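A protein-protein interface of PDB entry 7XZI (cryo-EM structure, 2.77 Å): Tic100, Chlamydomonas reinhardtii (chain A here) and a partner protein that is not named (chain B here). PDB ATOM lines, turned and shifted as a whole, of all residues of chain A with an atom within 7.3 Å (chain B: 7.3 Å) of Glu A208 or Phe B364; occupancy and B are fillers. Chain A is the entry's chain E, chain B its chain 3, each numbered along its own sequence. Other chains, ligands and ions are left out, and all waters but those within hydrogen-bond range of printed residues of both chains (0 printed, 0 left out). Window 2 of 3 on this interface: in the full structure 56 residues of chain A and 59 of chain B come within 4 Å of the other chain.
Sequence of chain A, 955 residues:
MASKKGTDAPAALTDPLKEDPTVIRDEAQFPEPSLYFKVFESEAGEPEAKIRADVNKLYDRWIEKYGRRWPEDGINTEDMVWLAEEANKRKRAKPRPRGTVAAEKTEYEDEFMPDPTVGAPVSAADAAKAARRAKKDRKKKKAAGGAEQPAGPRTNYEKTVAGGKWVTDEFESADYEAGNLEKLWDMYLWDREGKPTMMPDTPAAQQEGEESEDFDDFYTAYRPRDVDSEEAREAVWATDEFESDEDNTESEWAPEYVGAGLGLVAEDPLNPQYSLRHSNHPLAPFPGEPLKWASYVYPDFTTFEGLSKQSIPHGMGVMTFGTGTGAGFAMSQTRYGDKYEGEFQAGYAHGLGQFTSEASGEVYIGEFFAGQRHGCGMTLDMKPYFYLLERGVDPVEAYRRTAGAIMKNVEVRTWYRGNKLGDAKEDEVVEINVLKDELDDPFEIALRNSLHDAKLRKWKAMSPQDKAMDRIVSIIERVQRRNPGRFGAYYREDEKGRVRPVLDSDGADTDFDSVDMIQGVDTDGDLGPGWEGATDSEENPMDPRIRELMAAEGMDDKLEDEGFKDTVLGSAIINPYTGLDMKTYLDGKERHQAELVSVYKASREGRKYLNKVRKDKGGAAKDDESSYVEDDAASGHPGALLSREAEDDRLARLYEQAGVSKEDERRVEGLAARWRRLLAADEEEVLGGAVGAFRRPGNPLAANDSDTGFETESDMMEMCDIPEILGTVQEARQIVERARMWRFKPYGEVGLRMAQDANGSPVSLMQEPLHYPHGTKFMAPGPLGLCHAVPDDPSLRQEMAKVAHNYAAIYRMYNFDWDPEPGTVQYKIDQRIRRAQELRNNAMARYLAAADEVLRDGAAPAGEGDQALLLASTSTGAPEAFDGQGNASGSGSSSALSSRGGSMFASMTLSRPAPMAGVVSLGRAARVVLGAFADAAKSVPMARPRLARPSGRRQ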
ATOM      1  N   ALA A 205      24.520  -1.040 -17.796  1.00  0.00           N
ATOM      2  CA  ALA A 205      23.495  -0.306 -18.530  1.00  0.00           C
ATOM      3  C   ALA A 205      22.187  -1.083 -18.472  1.00  0.00           C
ATOM      4  O   ALA A 205      22.102  -2.206 -18.980  1.00  0.00           O
ATOM      5  CB  ALA A 205      23.935  -0.079 -19.973  1.00  0.00           C
ATOM      6  N   GLN A 206      21.170  -0.497 -17.837  1.00  0.00           N
ATOM      7  CA  GLN A 206      19.860  -1.140 -17.801  1.00  0.00           C
ATOM      8  C   GLN A 206      19.278  -1.267 -19.202  1.00  0.00           C
ATOM      9  O   GLN A 206      18.672  -2.291 -19.541  1.00  0.00           O
ATOM     10  CB  GLN A 206      18.917  -0.364 -16.883  1.00  0.00           C
ATOM     11  CG  GLN A 206      19.343  -0.363 -15.422  1.00  0.00           C
ATOM     12  CD  GLN A 206      19.421  -1.762 -14.834  1.00  0.00           C
ATOM     13  OE1 GLN A 206      18.682  -2.660 -15.236  1.00  0.00           O
ATOM     14  NE2 GLN A 206      20.325  -1.951 -13.881  1.00  0.00           N
ATOM     15  N   GLN A 207      19.449  -0.240 -20.029  1.00  0.00           N
ATOM     16  CA  GLN A 207      19.147  -0.373 -21.443  1.00  0.00           C
ATOM     17  C   GLN A 207      20.167  -1.296 -22.103  1.00  0.00           C
ATOM     18  O   GLN A 207      21.217  -1.611 -21.536  1.00  0.00           O
ATOM     19  CB  GLN A 207      19.135   0.993 -22.133  1.00  0.00           C
ATOM     20  CG  GLN A 207      20.444   1.764 -22.049  1.00  0.00           C
ATOM     21  CD  GLN A 207      20.607   2.505 -20.736  1.00  0.00           C
ATOM     22  OE1 GLN A 207      19.719   2.487 -19.884  1.00  0.00           O
ATOM     23  NE2 GLN A 207      21.749   3.163 -20.566  1.00  0.00           N
ATOM     24  N   GLU A 208      19.833  -1.745 -23.314  1.00  0.00           N
ATOM     25  CA  GLU A 208      20.594  -2.720 -24.094  1.00  0.00           C
ATOM     26  C   GLU A 208      20.541  -4.116 -23.488  1.00  0.00           C
ATOM     27  O   GLU A 208      21.224  -5.024 -23.979  1.00  0.00           O
ATOM     28  CB  GLU A 208      22.059  -2.299 -24.279  1.00  0.00           C
ATOM     29  CG  GLU A 208      22.243  -0.903 -24.856  1.00  0.00           C
ATOM     30  CD  GLU A 208      23.632  -0.347 -24.597  1.00  0.00           C
ATOM     31  OE1 GLU A 208      24.382  -0.964 -23.812  1.00  0.00           O
ATOM     32  OE2 GLU A 208      23.971   0.707 -25.174  1.00  0.00           O
ATOM     33  N   GLY A 209      19.746  -4.319 -22.436  1.00  0.00           N
ATOM     34  CA  GLY A 209      19.531  -5.628 -21.860  1.00  0.00           C
ATOM     35  C   GLY A 209      20.562  -6.092 -20.853  1.00  0.00           C
ATOM     36  O   GLY A 209      20.446  -7.219 -20.356  1.00  0.00           O
ATOM     37  N   GLU A 210      21.561  -5.275 -20.533  1.00  0.00           N
ATOM     38  CA  GLU A 210      22.602  -5.698 -19.607  1.00  0.00           C
ATOM     39  C   GLU A 210      22.140  -5.553 -18.161  1.00  0.00           C
ATOM     40  O   GLU A 210      21.300  -4.711 -17.833  1.00  0.00           O
ATOM     41  CB  GLU A 210      23.880  -4.892 -19.832  1.00  0.00           C
ATOM     42  CG  GLU A 210      24.470  -5.062 -21.220  1.00  0.00           C
ATOM     43  CD  GLU A 210      25.807  -4.370 -21.373  1.00  0.00           C
ATOM     44  OE1 GLU A 210      26.400  -3.984 -20.343  1.00  0.00           O
ATOM     45  OE2 GLU A 210      26.265  -4.212 -22.524  1.00  0.00           O
ATOM     46  N   GLU A 211      22.699  -6.395 -17.294  1.00  0.00           N
ATOM     47  CA  GLU A 211      22.393  -6.376 -15.871  1.00  0.00           C
ATOM     48  C   GLU A 211      23.683  -6.516 -15.076  1.00  0.00           C
ATOM     49  O   GLU A 211      24.680  -7.044 -15.572  1.00  0.00           O
ATOM     50  CB  GLU A 211      21.413  -7.490 -15.483  1.00  0.00           C
ATOM     51  CG  GLU A 211      20.032  -7.344 -16.096  1.00  0.00           C
ATOM     52  CD  GLU A 211      19.087  -8.446 -15.667  1.00  0.00           C
ATOM     53  OE1 GLU A 211      19.509  -9.312 -14.871  1.00  0.00           O
ATOM     54  OE2 GLU A 211      17.924  -8.448 -16.122  1.00  0.00           O
ATOM     55  N   PHE A 564      24.329  -7.676 -39.131  1.00  0.00           N
ATOM     56  CA  PHE A 564      23.650  -7.585 -37.842  1.00  0.00           C
ATOM     57  C   PHE A 564      24.480  -8.223 -36.734  1.00  0.00           C
ATOM     58  O   PHE A 564      24.618  -7.653 -35.643  1.00  0.00           O
ATOM     59  CB  PHE A 564      22.270  -8.239 -37.919  1.00  0.00           C
ATOM     60  CG  PHE A 564      21.524  -8.238 -36.612  1.00  0.00           C
ATOM     61  CD1 PHE A 564      20.876  -7.096 -36.171  1.00  0.00           C
ATOM     62  CD2 PHE A 564      21.471  -9.376 -35.825  1.00  0.00           C
ATOM     63  CE1 PHE A 564      20.190  -7.090 -34.971  1.00  0.00           C
ATOM     64  CE2 PHE A 564      20.786  -9.376 -34.623  1.00  0.00           C
ATOM     65  CZ  PHE A 564      20.145  -8.231 -34.196  1.00  0.00           C
ATOM     66  N   VAL A 568      26.059  -6.202 -33.507  1.00  0.00           N
ATOM     67  CA  VAL A 568      25.572  -6.568 -32.179  1.00  0.00           C
ATOM     68  C   VAL A 568      26.696  -7.066 -31.276  1.00  0.00           C
ATOM     69  O   VAL A 568      26.807  -6.643 -30.122  1.00  0.00           O
ATOM     70  CB  VAL A 568      24.442  -7.613 -32.297  1.00  0.00           C
ATOM     71  CG1 VAL A 568      24.119  -8.199 -30.935  1.00  0.00           C
ATOM     72  CG2 VAL A 568      23.204  -6.978 -32.902  1.00  0.00           C
ATOM     73  N   LEU A 569      27.559  -7.961 -31.770  1.00  0.00           N
ATOM     74  CA  LEU A 569      28.487  -8.673 -30.900  1.00  0.00           C
ATOM     75  C   LEU A 569      29.956  -8.329 -31.106  1.00  0.00           C
ATOM     76  O   LEU A 569      30.785  -8.770 -30.304  1.00  0.00           O
ATOM     77  CB  LEU A 569      28.317 -10.190 -31.073  1.00  0.00           C
ATOM     78  CG  LEU A 569      26.965 -10.778 -30.661  1.00  0.00           C
ATOM     79  CD1 LEU A 569      26.874 -12.249 -31.040  1.00  0.00           C
ATOM     80  CD2 LEU A 569      26.741 -10.593 -29.171  1.00  0.00           C
ATOM     81  N   MET A 582      33.831 -11.180 -29.734  1.00  0.00           N
ATOM     82  CA  MET A 582      32.829 -12.171 -29.357  1.00  0.00           C
ATOM     83  C   MET A 582      32.133 -12.778 -30.569  1.00  0.00           C
ATOM     84  O   MET A 582      31.730 -13.946 -30.522  1.00  0.00           O
ATOM     85  CB  MET A 582      31.797 -11.540 -28.418  1.00  0.00           C
ATOM     86  CG  MET A 582      30.718 -12.498 -27.943  1.00  0.00           C
ATOM     87  SD  MET A 582      29.506 -11.720 -26.863  1.00  0.00           S
ATOM     88  CE  MET A 582      30.532 -11.305 -25.457  1.00  0.00           C
ATOM     89  N   ASN B 358      22.744 -17.324 -29.489  1.00  0.00           N
ATOM     90  CA  ASN B 358      21.378 -16.894 -29.763  1.00  0.00           C
ATOM     91  C   ASN B 358      20.776 -16.134 -28.588  1.00  0.00           C
ATOM     92  O   ASN B 358      20.024 -15.177 -28.797  1.00  0.00           O
ATOM     93  CB  ASN B 358      20.510 -18.097 -30.122  1.00  0.00           C
ATOM     94  CG  ASN B 358      20.875 -18.692 -31.464  1.00  0.00           C
ATOM     95  OD1 ASN B 358      20.345 -18.287 -32.497  1.00  0.00           O
ATOM     96  ND2 ASN B 358      21.787 -19.656 -31.458  1.00  0.00           N
ATOM     97  N   PHE B 359      21.084 -16.539 -27.353  1.00  0.00           N
ATOM     98  CA  PHE B 359      20.578 -15.802 -26.199  1.00  0.00           C
ATOM     99  C   PHE B 359      21.118 -14.378 -26.177  1.00  0.00           C
ATOM    100  O   PHE B 359      20.371 -13.428 -25.915  1.00  0.00           O
ATOM    101  CB  PHE B 359      20.933 -16.531 -24.904  1.00  0.00           C
ATOM    102  CG  PHE B 359      20.714 -15.705 -23.668  1.00  0.00           C
ATOM    103  CD1 PHE B 359      19.433 -15.429 -23.223  1.00  0.00           C
ATOM    104  CD2 PHE B 359      21.789 -15.201 -22.956  1.00  0.00           C
ATOM    105  CE1 PHE B 359      19.228 -14.667 -22.089  1.00  0.00           C
ATOM    106  CE2 PHE B 359      21.590 -14.438 -21.823  1.00  0.00           C
ATOM    107  CZ  PHE B 359      20.308 -14.171 -21.389  1.00  0.00           C
ATOM    108  N   TYR B 360      22.413 -14.210 -26.454  1.00  0.00           N
ATOM    109  CA  TYR B 360      22.988 -12.871 -26.504  1.00  0.00           C
ATOM    110  C   TYR B 360      22.423 -12.055 -27.658  1.00  0.00           C
ATOM    111  O   TYR B 360      22.219 -10.845 -27.513  1.00  0.00           O
ATOM    112  CB  TYR B 360      24.511 -12.951 -26.601  1.00  0.00           C
ATOM    113  CG  TYR B 360      25.181 -13.269 -25.286  1.00  0.00           C
ATOM    114  CD1 TYR B 360      24.498 -13.116 -24.089  1.00  0.00           C
ATOM    115  CD2 TYR B 360      26.493 -13.715 -25.239  1.00  0.00           C
ATOM    116  CE1 TYR B 360      25.100 -13.401 -22.883  1.00  0.00           C
ATOM    117  CE2 TYR B 360      27.105 -14.003 -24.033  1.00  0.00           C
ATOM    118  CZ  TYR B 360      26.403 -13.844 -22.859  1.00  0.00           C
ATOM    119  OH  TYR B 360      26.999 -14.127 -21.653  1.00  0.00           O
ATOM    120  N   LEU B 361      22.175 -12.687 -28.808  1.00  0.00           N
ATOM    121  CA  LEU B 361      21.569 -11.961 -29.920  1.00  0.00           C
ATOM    122  C   LEU B 361      20.153 -11.510 -29.584  1.00  0.00           C
ATOM    123  O   LEU B 361      19.742 -10.406 -29.958  1.00  0.00           O
ATOM    124  CB  LEU B 361      21.573 -12.822 -31.183  1.00  0.00           C
ATOM    125  CG  LEU B 361      22.893 -12.888 -31.954  1.00  0.00           C
ATOM    126  CD1 LEU B 361      22.766 -13.785 -33.176  1.00  0.00           C
ATOM    127  CD2 LEU B 361      23.332 -11.493 -32.359  1.00  0.00           C
ATOM    128  N   ALA B 362      19.391 -12.351 -28.884  1.00  0.00           N
ATOM    129  CA  ALA B 362      18.014 -12.001 -28.553  1.00  0.00           C
ATOM    130  C   ALA B 362      17.943 -10.945 -27.457  1.00  0.00           C
ATOM    131  O   ALA B 362      17.090 -10.053 -27.515  1.00  0.00           O
ATOM    132  CB  ALA B 362      17.239 -13.249 -28.136  1.00  0.00           C
ATOM    133  N   SER B 363      18.823 -11.023 -26.458  1.00  0.00           N
ATOM    134  CA  SER B 363      18.764 -10.087 -25.339  1.00  0.00           C
ATOM    135  C   SER B 363      19.311  -8.717 -25.730  1.00  0.00           C
ATOM    136  O   SER B 363      18.603  -7.708 -25.649  1.00  0.00           O
ATOM    137  CB  SER B 363      19.531 -10.652 -24.141  1.00  0.00           C
ATOM    138  OG  SER B 363      18.938 -11.854 -23.681  1.00  0.00           O
ATOM    139  N   PHE B 364      20.572  -8.667 -26.160  1.00  0.00           N
ATOM    140  CA  PHE B 364      21.202  -7.403 -26.519  1.00  0.00           C
ATOM    141  C   PHE B 364      20.663  -6.821 -27.818  1.00  0.00           C
ATOM    142  O   PHE B 364      20.893  -5.638 -28.088  1.00  0.00           O
ATOM    143  CB  PHE B 364      22.716  -7.590 -26.617  1.00  0.00           C
ATOM    144  CG  PHE B 364      23.341  -8.117 -25.357  1.00  0.00           C
ATOM    145  CD1 PHE B 364      22.851  -7.745 -24.117  1.00  0.00           C
ATOM    146  CD2 PHE B 364      24.408  -8.995 -25.413  1.00  0.00           C
ATOM    147  CE1 PHE B 364      23.420  -8.230 -22.957  1.00  0.00           C
ATOM    148  CE2 PHE B 364      24.981  -9.484 -24.256  1.00  0.00           C
ATOM    149  CZ  PHE B 364      24.486  -9.101 -23.026  1.00  0.00           C
ATOM    150  N   GLY B 365      19.972  -7.615 -28.623  1.00  0.00           N
ATOM    151  CA  GLY B 365      19.300  -7.157 -29.819  1.00  0.00           C
ATOM    152  C   GLY B 365      17.831  -6.883 -29.577  1.00  0.00           C
ATOM    153  O   GLY B 365      17.403  -6.608 -28.450  1.00  0.00           O
ATOM    154  N   GLY B 366      17.044  -6.956 -30.646  1.00  0.00           N
ATOM    155  CA  GLY B 366      15.619  -6.720 -30.535  1.00  0.00           C
ATOM    156  C   GLY B 366      14.768  -7.600 -31.427  1.00  0.00           C
ATOM    157  O   GLY B 366      13.631  -7.242 -31.750  1.00  0.00           O
ATOM    158  N   LEU B 367      15.298  -8.751 -31.828  1.00  0.00           N
ATOM    159  CA  LEU B 367      14.607  -9.655 -32.739  1.00  0.00           C
ATOM    160  C   LEU B 367      14.111 -10.880 -31.982  1.00  0.00           C
ATOM    161  O   LEU B 367      14.882 -11.531 -31.267  1.00  0.00           O
ATOM    162  CB  LEU B 367      15.526 -10.073 -33.888  1.00  0.00           C
ATOM    163  CG  LEU B 367      16.126  -8.919 -34.695  1.00  0.00           C
ATOM    164  CD1 LEU B 367      16.902  -9.431 -35.899  1.00  0.00           C
ATOM    165  CD2 LEU B 367      15.038  -7.953 -35.130  1.00  0.00           C
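N of Glu A210 sits close to O of Ala A205, 3.5 Å away.
Of the 10 printed residues of chain B, 4 touch a printed residue of chain A. Printed residues of chain B that touch a printed residue of chain A: Tyr B360, Leu B361, Phe B364 and Leu B367. Hydrophobic or aromatic side chains of chain B that line the printed part of chain A: Tyr B360, Leu B361, Phe B364 and Leu B367. Of the 11 printed residues of chain A, 6 touch a printed residue of chain B. Among the printed residues, 6 pairs touch across the chains. Among the printed residues, no Asp or Glu carboxylate lies within 4 Å of a Lys or Arg side-chain nitrogen of the other chain.
Glu A208 touches one residue of chain B. Of the printed residues of chain B, Glu A210 touches Phe B364. Printed residues of chain B within 4 Å of Leu A569: Leu B361 (3.9 Å). Printed residues of chain B within 4 Å of Met A582: Tyr B360 (3.96 Å). Of the printed residues of chain A, Leu B361 touches Val A568 and Leu A569. Ser B363 touches none of the printed residues of chain A. Printed residues of chain A within 4 Å of Phe B364: Glu A208 and Glu A210. Gly B366 touches none of the printed residues of chain A.
CD1 of Phe B364 touches O of Glu A208, 3.2 Å away. Glu A210 touches Phe B364 (CG to CE1, 3.8 Å). CD1 of Leu B367 touches CZ of Phe A564, 3.9 Å away. CG1 of Val A568 touches CD2 of Leu B361 (3.7 Å). CD2 of Leu B361 touches CD1 of Leu A569 (3.9 Å). Met A582 touches Tyr B360 (SD to CD2, 3.96 Å).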
